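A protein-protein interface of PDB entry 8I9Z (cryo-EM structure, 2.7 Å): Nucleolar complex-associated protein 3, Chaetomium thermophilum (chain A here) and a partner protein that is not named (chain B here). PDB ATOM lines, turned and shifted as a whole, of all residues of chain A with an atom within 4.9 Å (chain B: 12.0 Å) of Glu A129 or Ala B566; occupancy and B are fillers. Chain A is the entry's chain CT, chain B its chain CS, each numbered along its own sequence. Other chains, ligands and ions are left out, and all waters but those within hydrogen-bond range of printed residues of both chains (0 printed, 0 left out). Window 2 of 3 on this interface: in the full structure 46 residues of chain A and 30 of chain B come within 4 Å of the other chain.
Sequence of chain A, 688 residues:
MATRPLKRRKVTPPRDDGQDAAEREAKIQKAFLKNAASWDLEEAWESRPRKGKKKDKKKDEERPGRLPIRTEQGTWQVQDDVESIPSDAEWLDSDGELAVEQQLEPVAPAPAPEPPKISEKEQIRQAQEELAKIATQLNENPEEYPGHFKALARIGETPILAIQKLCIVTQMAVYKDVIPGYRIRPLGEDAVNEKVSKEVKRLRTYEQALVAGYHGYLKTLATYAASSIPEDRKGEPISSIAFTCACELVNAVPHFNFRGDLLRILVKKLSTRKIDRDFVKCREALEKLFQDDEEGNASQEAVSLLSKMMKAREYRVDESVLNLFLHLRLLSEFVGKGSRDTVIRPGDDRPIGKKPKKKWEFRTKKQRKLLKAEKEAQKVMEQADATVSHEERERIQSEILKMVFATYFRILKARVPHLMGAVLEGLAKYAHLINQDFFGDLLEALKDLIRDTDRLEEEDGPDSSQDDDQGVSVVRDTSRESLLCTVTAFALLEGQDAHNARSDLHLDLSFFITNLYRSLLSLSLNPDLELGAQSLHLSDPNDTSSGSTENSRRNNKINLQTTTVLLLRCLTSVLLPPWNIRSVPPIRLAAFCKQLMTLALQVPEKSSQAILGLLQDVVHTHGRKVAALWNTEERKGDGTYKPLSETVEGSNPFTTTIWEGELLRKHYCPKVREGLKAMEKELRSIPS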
ATOM      1  N   ARG A 125     -31.093  -8.646  -6.608  1.00  0.00           N
ATOM      2  CA  ARG A 125     -31.450  -9.960  -6.088  1.00  0.00           C
ATOM      3  C   ARG A 125     -31.697 -10.939  -7.222  1.00  0.00           C
ATOM      4  O   ARG A 125     -31.113 -12.024  -7.245  1.00  0.00           O
ATOM      5  CB  ARG A 125     -32.680  -9.864  -5.181  1.00  0.00           C
ATOM      6  CG  ARG A 125     -33.531 -11.130  -5.162  1.00  0.00           C
ATOM      7  CD  ARG A 125     -33.518 -11.842  -3.824  1.00  0.00           C
ATOM      8  NE  ARG A 125     -34.615 -12.799  -3.730  1.00  0.00           N
ATOM      9  CZ  ARG A 125     -34.862 -13.560  -2.672  1.00  0.00           C
ATOM     10  NH1 ARG A 125     -34.101 -13.509  -1.592  1.00  0.00           N
ATOM     11  NH2 ARG A 125     -35.895 -14.396  -2.703  1.00  0.00           N
ATOM     12  N   GLN A 126     -32.497 -10.535  -8.216  1.00  0.00           N
ATOM     13  CA  GLN A 126     -33.013 -11.481  -9.204  1.00  0.00           C
ATOM     14  C   GLN A 126     -31.910 -12.009 -10.109  1.00  0.00           C
ATOM     15  O   GLN A 126     -32.090 -13.029 -10.783  1.00  0.00           O
ATOM     16  CB  GLN A 126     -34.125 -10.818 -10.022  1.00  0.00           C
ATOM     17  CG  GLN A 126     -33.665  -9.841 -11.095  1.00  0.00           C
ATOM     18  CD  GLN A 126     -33.546 -10.481 -12.468  1.00  0.00           C
ATOM     19  OE1 GLN A 126     -34.501 -11.067 -12.977  1.00  0.00           O
ATOM     20  NE2 GLN A 126     -32.368 -10.371 -13.073  1.00  0.00           N
ATOM     21  N   ALA A 127     -30.767 -11.326 -10.141  1.00  0.00           N
ATOM     22  CA  ALA A 127     -29.608 -11.859 -10.842  1.00  0.00           C
ATOM     23  C   ALA A 127     -29.023 -13.063 -10.114  1.00  0.00           C
ATOM     24  O   ALA A 127     -28.564 -14.012 -10.754  1.00  0.00           O
ATOM     25  CB  ALA A 127     -28.553 -10.771 -11.005  1.00  0.00           C
ATOM     26  N   GLN A 128     -29.040 -13.044  -8.778  1.00  0.00           N
ATOM     27  CA  GLN A 128     -28.311 -14.046  -8.003  1.00  0.00           C
ATOM     28  C   GLN A 128     -28.878 -15.449  -8.194  1.00  0.00           C
ATOM     29  O   GLN A 128     -28.115 -16.420  -8.243  1.00  0.00           O
ATOM     30  CB  GLN A 128     -28.292 -13.665  -6.524  1.00  0.00           C
ATOM     31  CG  GLN A 128     -27.939 -12.213  -6.273  1.00  0.00           C
ATOM     32  CD  GLN A 128     -27.302 -11.987  -4.920  1.00  0.00           C
ATOM     33  OE1 GLN A 128     -26.987 -12.936  -4.203  1.00  0.00           O
ATOM     34  NE2 GLN A 128     -27.105 -10.724  -4.563  1.00  0.00           N
ATOM     35  N   GLU A 129     -30.204 -15.593  -8.294  1.00  0.00           N
ATOM     36  CA  GLU A 129     -30.729 -16.890  -8.712  1.00  0.00           C
ATOM     37  C   GLU A 129     -30.426 -17.153 -10.178  1.00  0.00           C
ATOM     38  O   GLU A 129     -30.148 -18.295 -10.560  1.00  0.00           O
ATOM     39  CB  GLU A 129     -32.241 -17.040  -8.450  1.00  0.00           C
ATOM     40  CG  GLU A 129     -32.814 -16.743  -7.041  1.00  0.00           C
ATOM     41  CD  GLU A 129     -32.746 -15.301  -6.595  1.00  0.00           C
ATOM     42  OE1 GLU A 129     -33.302 -14.981  -5.523  1.00  0.00           O
ATOM     43  OE2 GLU A 129     -32.208 -14.476  -7.342  1.00  0.00           O
ATOM     44  N   GLU A 130     -30.467 -16.116 -11.018  1.00  0.00           N
ATOM     45  CA  GLU A 130     -30.199 -16.342 -12.434  1.00  0.00           C
ATOM     46  C   GLU A 130     -28.710 -16.552 -12.693  1.00  0.00           C
ATOM     47  O   GLU A 130     -28.343 -17.201 -13.677  1.00  0.00           O
ATOM     48  CB  GLU A 130     -30.764 -15.193 -13.275  1.00  0.00           C
ATOM     49  CG  GLU A 130     -29.759 -14.181 -13.794  1.00  0.00           C
ATOM     50  CD  GLU A 130     -30.347 -13.282 -14.866  1.00  0.00           C
ATOM     51  OE1 GLU A 130     -31.148 -13.777 -15.687  1.00  0.00           O
ATOM     52  OE2 GLU A 130     -30.014 -12.079 -14.884  1.00  0.00           O
ATOM     53  N   LEU A 131     -27.842 -16.016 -11.829  1.00  0.00           N
ATOM     54  CA  LEU A 131     -26.440 -16.419 -11.855  1.00  0.00           C
ATOM     55  C   LEU A 131     -26.297 -17.869 -11.416  1.00  0.00           C
ATOM     56  O   LEU A 131     -25.540 -18.641 -12.014  1.00  0.00           O
ATOM     57  CB  LEU A 131     -25.599 -15.513 -10.951  1.00  0.00           C
ATOM     58  CG  LEU A 131     -24.833 -14.285 -11.467  1.00  0.00           C
ATOM     59  CD1 LEU A 131     -25.736 -13.231 -12.048  1.00  0.00           C
ATOM     60  CD2 LEU A 131     -23.999 -13.677 -10.369  1.00  0.00           C
ATOM     61  N   ALA A 132     -27.020 -18.256 -10.363  1.00  0.00           N
ATOM     62  CA  ALA A 132     -26.942 -19.622  -9.858  1.00  0.00           C
ATOM     63  C   ALA A 132     -27.692 -20.590 -10.762  1.00  0.00           C
ATOM     64  O   ALA A 132     -27.454 -21.802 -10.725  1.00  0.00           O
ATOM     65  CB  ALA A 132     -27.489 -19.684  -8.432  1.00  0.00           C
ATOM     66  N   LYS A 133     -28.624 -20.073 -11.561  1.00  0.00           N
ATOM     67  CA  LYS A 133     -29.346 -20.902 -12.516  1.00  0.00           C
ATOM     68  C   LYS A 133     -28.406 -21.437 -13.583  1.00  0.00           C
ATOM     69  O   LYS A 133     -28.454 -22.621 -13.914  1.00  0.00           O
ATOM     70  CB  LYS A 133     -30.486 -20.117 -13.169  1.00  0.00           C
ATOM     71  CG  LYS A 133     -31.854 -20.402 -12.568  1.00  0.00           C
ATOM     72  CD  LYS A 133     -32.870 -19.332 -12.932  1.00  0.00           C
ATOM     73  CE  LYS A 133     -33.596 -18.831 -11.693  1.00  0.00           C
ATOM     74  NZ  LYS A 133     -33.863 -17.368 -11.742  1.00  0.00           N
ATOM     75  N   ASP B 551     -34.707 -31.954   1.362  1.00  0.00           N
ATOM     76  CA  ASP B 551     -33.429 -31.705   2.011  1.00  0.00           C
ATOM     77  C   ASP B 551     -33.712 -31.267   3.440  1.00  0.00           C
ATOM     78  O   ASP B 551     -34.333 -30.221   3.660  1.00  0.00           O
ATOM     79  CB  ASP B 551     -32.635 -30.635   1.262  1.00  0.00           C
ATOM     80  CG  ASP B 551     -32.354 -31.019  -0.179  1.00  0.00           C
ATOM     81  OD1 ASP B 551     -32.595 -32.188  -0.542  1.00  0.00           O
ATOM     82  OD2 ASP B 551     -31.896 -30.148  -0.949  1.00  0.00           O
ATOM     83  N   SER B 563     -33.202 -18.167  -2.829  1.00  0.00           N
ATOM     84  CA  SER B 563     -33.401 -19.609  -2.888  1.00  0.00           C
ATOM     85  C   SER B 563     -32.263 -20.338  -2.197  1.00  0.00           C
ATOM     86  O   SER B 563     -31.256 -19.730  -1.848  1.00  0.00           O
ATOM     87  CB  SER B 563     -33.515 -20.081  -4.335  1.00  0.00           C
ATOM     88  OG  SER B 563     -32.946 -21.368  -4.489  1.00  0.00           O
ATOM     89  N   LYS B 564     -32.432 -21.645  -1.990  1.00  0.00           N
ATOM     90  CA  LYS B 564     -31.365 -22.436  -1.391  1.00  0.00           C
ATOM     91  C   LYS B 564     -30.218 -22.647  -2.370  1.00  0.00           C
ATOM     92  O   LYS B 564     -29.054 -22.727  -1.962  1.00  0.00           O
ATOM     93  CB  LYS B 564     -31.909 -23.778  -0.906  1.00  0.00           C
ATOM     94  CG  LYS B 564     -33.148 -23.666  -0.039  1.00  0.00           C
ATOM     95  CD  LYS B 564     -33.750 -25.036   0.236  1.00  0.00           C
ATOM     96  CE  LYS B 564     -35.057 -24.923   1.002  1.00  0.00           C
ATOM     97  NZ  LYS B 564     -35.715 -26.248   1.175  1.00  0.00           N
ATOM     98  N   ARG B 565     -30.532 -22.757  -3.664  1.00  0.00           N
ATOM     99  CA  ARG B 565     -29.486 -22.869  -4.677  1.00  0.00           C
ATOM    100  C   ARG B 565     -28.678 -21.583  -4.770  1.00  0.00           C
ATOM    101  O   ARG B 565     -27.446 -21.614  -4.861  1.00  0.00           O
ATOM    102  CB  ARG B 565     -30.106 -23.212  -6.030  1.00  0.00           C
ATOM    103  CG  ARG B 565     -29.152 -23.897  -6.983  1.00  0.00           C
ATOM    104  CD  ARG B 565     -29.842 -24.270  -8.276  1.00  0.00           C
ATOM    105  NE  ARG B 565     -30.853 -23.289  -8.647  1.00  0.00           N
ATOM    106  CZ  ARG B 565     -31.608 -23.370  -9.733  1.00  0.00           C
ATOM    107  NH1 ARG B 565     -31.479 -24.366 -10.592  1.00  0.00           N
ATOM    108  NH2 ARG B 565     -32.516 -22.426  -9.963  1.00  0.00           N
ATOM    109  N   ALA B 566     -29.362 -20.438  -4.754  1.00  0.00           N
ATOM    110  CA  ALA B 566     -28.666 -19.159  -4.788  1.00  0.00           C
ATOM    111  C   ALA B 566     -27.900 -18.917  -3.496  1.00  0.00           C
ATOM    112  O   ALA B 566     -26.821 -18.316  -3.509  1.00  0.00           O
ATOM    113  CB  ALA B 566     -29.659 -18.027  -5.047  1.00  0.00           C
ATOM    114  N   ARG B 567     -28.446 -19.365  -2.367  1.00  0.00           N
ATOM    115  CA  ARG B 567     -27.712 -19.258  -1.113  1.00  0.00           C
ATOM    116  C   ARG B 567     -26.514 -20.195  -1.099  1.00  0.00           C
ATOM    117  O   ARG B 567     -25.443 -19.837  -0.598  1.00  0.00           O
ATOM    118  CB  ARG B 567     -28.632 -19.550   0.071  1.00  0.00           C
ATOM    119  CG  ARG B 567     -29.310 -18.321   0.645  1.00  0.00           C
ATOM    120  CD  ARG B 567     -30.450 -18.704   1.567  1.00  0.00           C
ATOM    121  NE  ARG B 567     -31.641 -19.101   0.828  1.00  0.00           N
ATOM    122  CZ  ARG B 567     -32.786 -19.457   1.394  1.00  0.00           C
ATOM    123  NH1 ARG B 567     -32.926 -19.483   2.710  1.00  0.00           N
ATOM    124  NH2 ARG B 567     -33.814 -19.800   0.623  1.00  0.00           N
ATOM    125  N   GLY B 568     -26.679 -21.400  -1.645  1.00  0.00           N
ATOM    126  CA  GLY B 568     -25.583 -22.355  -1.655  1.00  0.00           C
ATOM    127  C   GLY B 568     -24.444 -21.940  -2.566  1.00  0.00           C
ATOM    128  O   GLY B 568     -23.271 -22.123  -2.233  1.00  0.00           O
ATOM    129  N   PHE B 569     -24.775 -21.386  -3.737  1.00  0.00           N
ATOM    130  CA  PHE B 569     -23.738 -21.043  -4.705  1.00  0.00           C
ATOM    131  C   PHE B 569     -22.927 -19.859  -4.198  1.00  0.00           C
ATOM    132  O   PHE B 569     -21.699 -19.835  -4.326  1.00  0.00           O
ATOM    133  CB  PHE B 569     -24.378 -20.723  -6.063  1.00  0.00           C
ATOM    134  CG  PHE B 569     -23.422 -20.166  -7.111  1.00  0.00           C
ATOM    135  CD1 PHE B 569     -23.872 -19.280  -8.063  1.00  0.00           C
ATOM    136  CD2 PHE B 569     -22.137 -20.673  -7.256  1.00  0.00           C
ATOM    137  CE1 PHE B 569     -23.024 -18.804  -9.051  1.00  0.00           C
ATOM    138  CE2 PHE B 569     -21.290 -20.201  -8.234  1.00  0.00           C
ATOM    139  CZ  PHE B 569     -21.737 -19.271  -9.137  1.00  0.00           C
ATOM    140  N   PHE B 570     -23.587 -18.886  -3.584  1.00  0.00           N
ATOM    141  CA  PHE B 570     -22.896 -17.697  -3.122  1.00  0.00           C
ATOM    142  C   PHE B 570     -22.366 -17.850  -1.706  1.00  0.00           C
ATOM    143  O   PHE B 570     -21.796 -16.901  -1.162  1.00  0.00           O
ATOM    144  CB  PHE B 570     -23.809 -16.474  -3.234  1.00  0.00           C
ATOM    145  CG  PHE B 570     -24.053 -16.045  -4.653  1.00  0.00           C
ATOM    146  CD1 PHE B 570     -24.962 -16.718  -5.448  1.00  0.00           C
ATOM    147  CD2 PHE B 570     -23.317 -15.020  -5.216  1.00  0.00           C
ATOM    148  CE1 PHE B 570     -25.173 -16.345  -6.749  1.00  0.00           C
ATOM    149  CE2 PHE B 570     -23.520 -14.652  -6.525  1.00  0.00           C
ATOM    150  CZ  PHE B 570     -24.450 -15.316  -7.289  1.00  0.00           C
ATOM    151  N   SER B 571     -22.533 -19.025  -1.109  1.00  0.00           N
ATOM    152  CA  SER B 571     -21.802 -19.402   0.091  1.00  0.00           C
ATOM    153  C   SER B 571     -20.471 -20.056  -0.236  1.00  0.00           C
ATOM    154  O   SER B 571     -19.792 -20.540   0.674  1.00  0.00           O
ATOM    155  CB  SER B 571     -22.645 -20.342   0.958  1.00  0.00           C
ATOM    156  OG  SER B 571     -22.722 -21.634   0.383  1.00  0.00           O
ATOM    157  N   GLN B 572     -20.092 -20.087  -1.513  1.00  0.00           N
ATOM    158  CA  GLN B 572     -18.792 -20.595  -1.918  1.00  0.00           C
ATOM    159  C   GLN B 572     -17.687 -19.655  -1.452  1.00  0.00           C
ATOM    160  O   GLN B 572     -17.918 -18.485  -1.133  1.00  0.00           O
ATOM    161  CB  GLN B 572     -18.741 -20.771  -3.435  1.00  0.00           C
ATOM    162  CG  GLN B 572     -19.321 -22.091  -3.922  1.00  0.00           C
ATOM    163  CD  GLN B 572     -19.056 -22.345  -5.392  1.00  0.00           C
ATOM    164  OE1 GLN B 572     -18.517 -21.491  -6.095  1.00  0.00           O
ATOM    165  NE2 GLN B 572     -19.432 -23.527  -5.865  1.00  0.00           N
ATOM    166  N   ASP B 573     -16.466 -20.196  -1.410  1.00  0.00           N
ATOM    167  CA  ASP B 573     -15.334 -19.482  -0.828  1.00  0.00           C
ATOM    168  C   ASP B 573     -14.989 -18.227  -1.617  1.00  0.00           C
ATOM    169  O   ASP B 573     -14.668 -17.190  -1.029  1.00  0.00           O
ATOM    170  CB  ASP B 573     -14.122 -20.410  -0.751  1.00  0.00           C
ATOM    171  CG  ASP B 573     -13.830 -20.877   0.662  1.00  0.00           C
ATOM    172  OD1 ASP B 573     -12.885 -21.672   0.843  1.00  0.00           O
ATOM    173  OD2 ASP B 573     -14.549 -20.452   1.591  1.00  0.00           O
ATOM    174  N   VAL B 574     -15.069 -18.297  -2.945  1.00  0.00           N
ATOM    175  CA  VAL B 574     -14.566 -17.209  -3.779  1.00  0.00           C
ATOM    176  C   VAL B 574     -15.444 -15.968  -3.631  1.00  0.00           C
ATOM    177  O   VAL B 574     -14.955 -14.833  -3.660  1.00  0.00           O
ATOM    178  CB  VAL B 574     -14.448 -17.682  -5.242  1.00  0.00           C
ATOM    179  CG1 VAL B 574     -15.710 -18.408  -5.687  1.00  0.00           C
ATOM    180  CG2 VAL B 574     -14.059 -16.550  -6.180  1.00  0.00           C
ATOM    181  N   PHE B 575     -16.747 -16.161  -3.414  1.00  0.00           N
ATOM    182  CA  PHE B 575     -17.626 -15.012  -3.223  1.00  0.00           C
ATOM    183  C   PHE B 575     -17.519 -14.426  -1.820  1.00  0.00           C
ATOM    184  O   PHE B 575     -18.054 -13.342  -1.564  1.00  0.00           O
ATOM    185  CB  PHE B 575     -19.077 -15.383  -3.526  1.00  0.00           C
ATOM    186  CG  PHE B 575     -19.296 -15.891  -4.919  1.00  0.00           C
ATOM    187  CD1 PHE B 575     -19.481 -15.006  -5.967  1.00  0.00           C
ATOM    188  CD2 PHE B 575     -19.335 -17.248  -5.178  1.00  0.00           C
ATOM    189  CE1 PHE B 575     -19.691 -15.462  -7.250  1.00  0.00           C
ATOM    190  CE2 PHE B 575     -19.543 -17.709  -6.460  1.00  0.00           C
ATOM    191  CZ  PHE B 575     -19.721 -16.815  -7.497  1.00  0.00           C
ATOM    192  N   GLN B 576     -16.863 -15.122  -0.890  1.00  0.00           N
ATOM    193  CA  GLN B 576     -16.813 -14.614   0.477  1.00  0.00           C
ATOM    194  C   GLN B 576     -15.573 -13.759   0.722  1.00  0.00           C
ATOM    195  O   GLN B 576     -15.634 -12.778   1.469  1.00  0.00           O
ATOM    196  CB  GLN B 576     -16.888 -15.772   1.471  1.00  0.00           C
ATOM    197  CG  GLN B 576     -18.285 -16.121   2.071  1.00  0.00           C
ATOM    198  CD  GLN B 576     -19.125 -14.936   2.581  1.00  0.00           C
ATOM    199  OE1 GLN B 576     -19.578 -14.078   1.820  1.00  0.00           O
ATOM    200  NE2 GLN B 576     -19.332 -14.899   3.893  1.00  0.00           N
ATOM    201  N   LEU B 581     -19.447  -6.256  -2.300  1.00  0.00           N
ATOM    202  CA  LEU B 581     -20.193  -6.786  -3.440  1.00  0.00           C
ATOM    203  C   LEU B 581     -21.185  -5.772  -4.004  1.00  0.00           C
ATOM    204  O   LEU B 581     -22.288  -5.609  -3.480  1.00  0.00           O
ATOM    205  CB  LEU B 581     -20.941  -8.056  -3.039  1.00  0.00           C
ATOM    206  CG  LEU B 581     -20.111  -9.190  -2.445  1.00  0.00           C
ATOM    207  CD1 LEU B 581     -21.025 -10.308  -1.972  1.00  0.00           C
ATOM    208  CD2 LEU B 581     -19.114  -9.696  -3.469  1.00  0.00           C
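No residue of chain B comes within 4 Å of Arg A125.
No residue of chain B comes within 4 Å of Ala A127.
Gln A128 touches just these residues of chain B: Ala B566 (3.9 Å) and Phe B570 (3.3 Å).
Glu A129 touches just one residue of chain B: Ala B566.
Of the printed residues of chain B, Leu A131 touches Phe B569 and Phe B570.
Of chain B, only Ala B566 (3.9 Å) and Phe B569 (3.6 Å) come within 4 Å of Ala A132.
Lys A133 touches one residue of chain B.
Lys B564 touches none of the printed residues of chain A.
Printed residues of chain A within 4 Å of Arg B565: Lys A133 (3.4 Å).
Ala B566 touches three residues of chain A.
Of the printed residues of chain A, Phe B569 touches Leu A131 (3.9 Å) and Ala A132 (3.6 Å).
Of the printed residues of chain A, Phe B570 touches Gln A128 and Leu A131.
Asp B573 touches none of the printed residues of chain A.
The nearest printed residue of chain A that does not touch Arg B565 is Ala A132 (4.1 Å).
OG of Ser B563 lies within hydrogen-bond range of N of Arg B565.
OE1 of Glu A129 is in salt-bridge range of NE of Arg A125 (3.1 Å).
Hydrophobic or aromatic side chains of chain B that line the printed part of chain A: Ala B566, Phe B569 and Phe B570.
Of the 9 printed residues of chain A, 5 touch a printed residue of chain B.
Printed residues of chain A that touch a printed residue of chain B: Gln A128, Glu A129, Leu A131, Ala A132 and Lys A133.
Hydrophobic or aromatic side chains of chain A within 4 Å of the printed part of chain B: Leu A131 and Ala A132.
Among the printed residues, 8 pairs touch across the chains.
Among the printed residues, no Asp or Glu carboxylate lies within 4 Å of a Lys or Arg side-chain nitrogen of the other chain.
Among the printed residues, pairs that only touch across the chains: Gln A128 with Ala B566 (3.9 Å), Gln A128 with Phe B570 (3.3 Å), Glu A129 with Ala B566 (3.9 Å), Leu A131 with Phe B569 (3.9 Å), Leu A131 with Phe B570 (3.5 Å), Ala A132 with Ala B566 (3.9 Å), Ala A132 with Phe B569 (3.6 Å) and Lys A133 with Arg B565 (3.4 Å).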
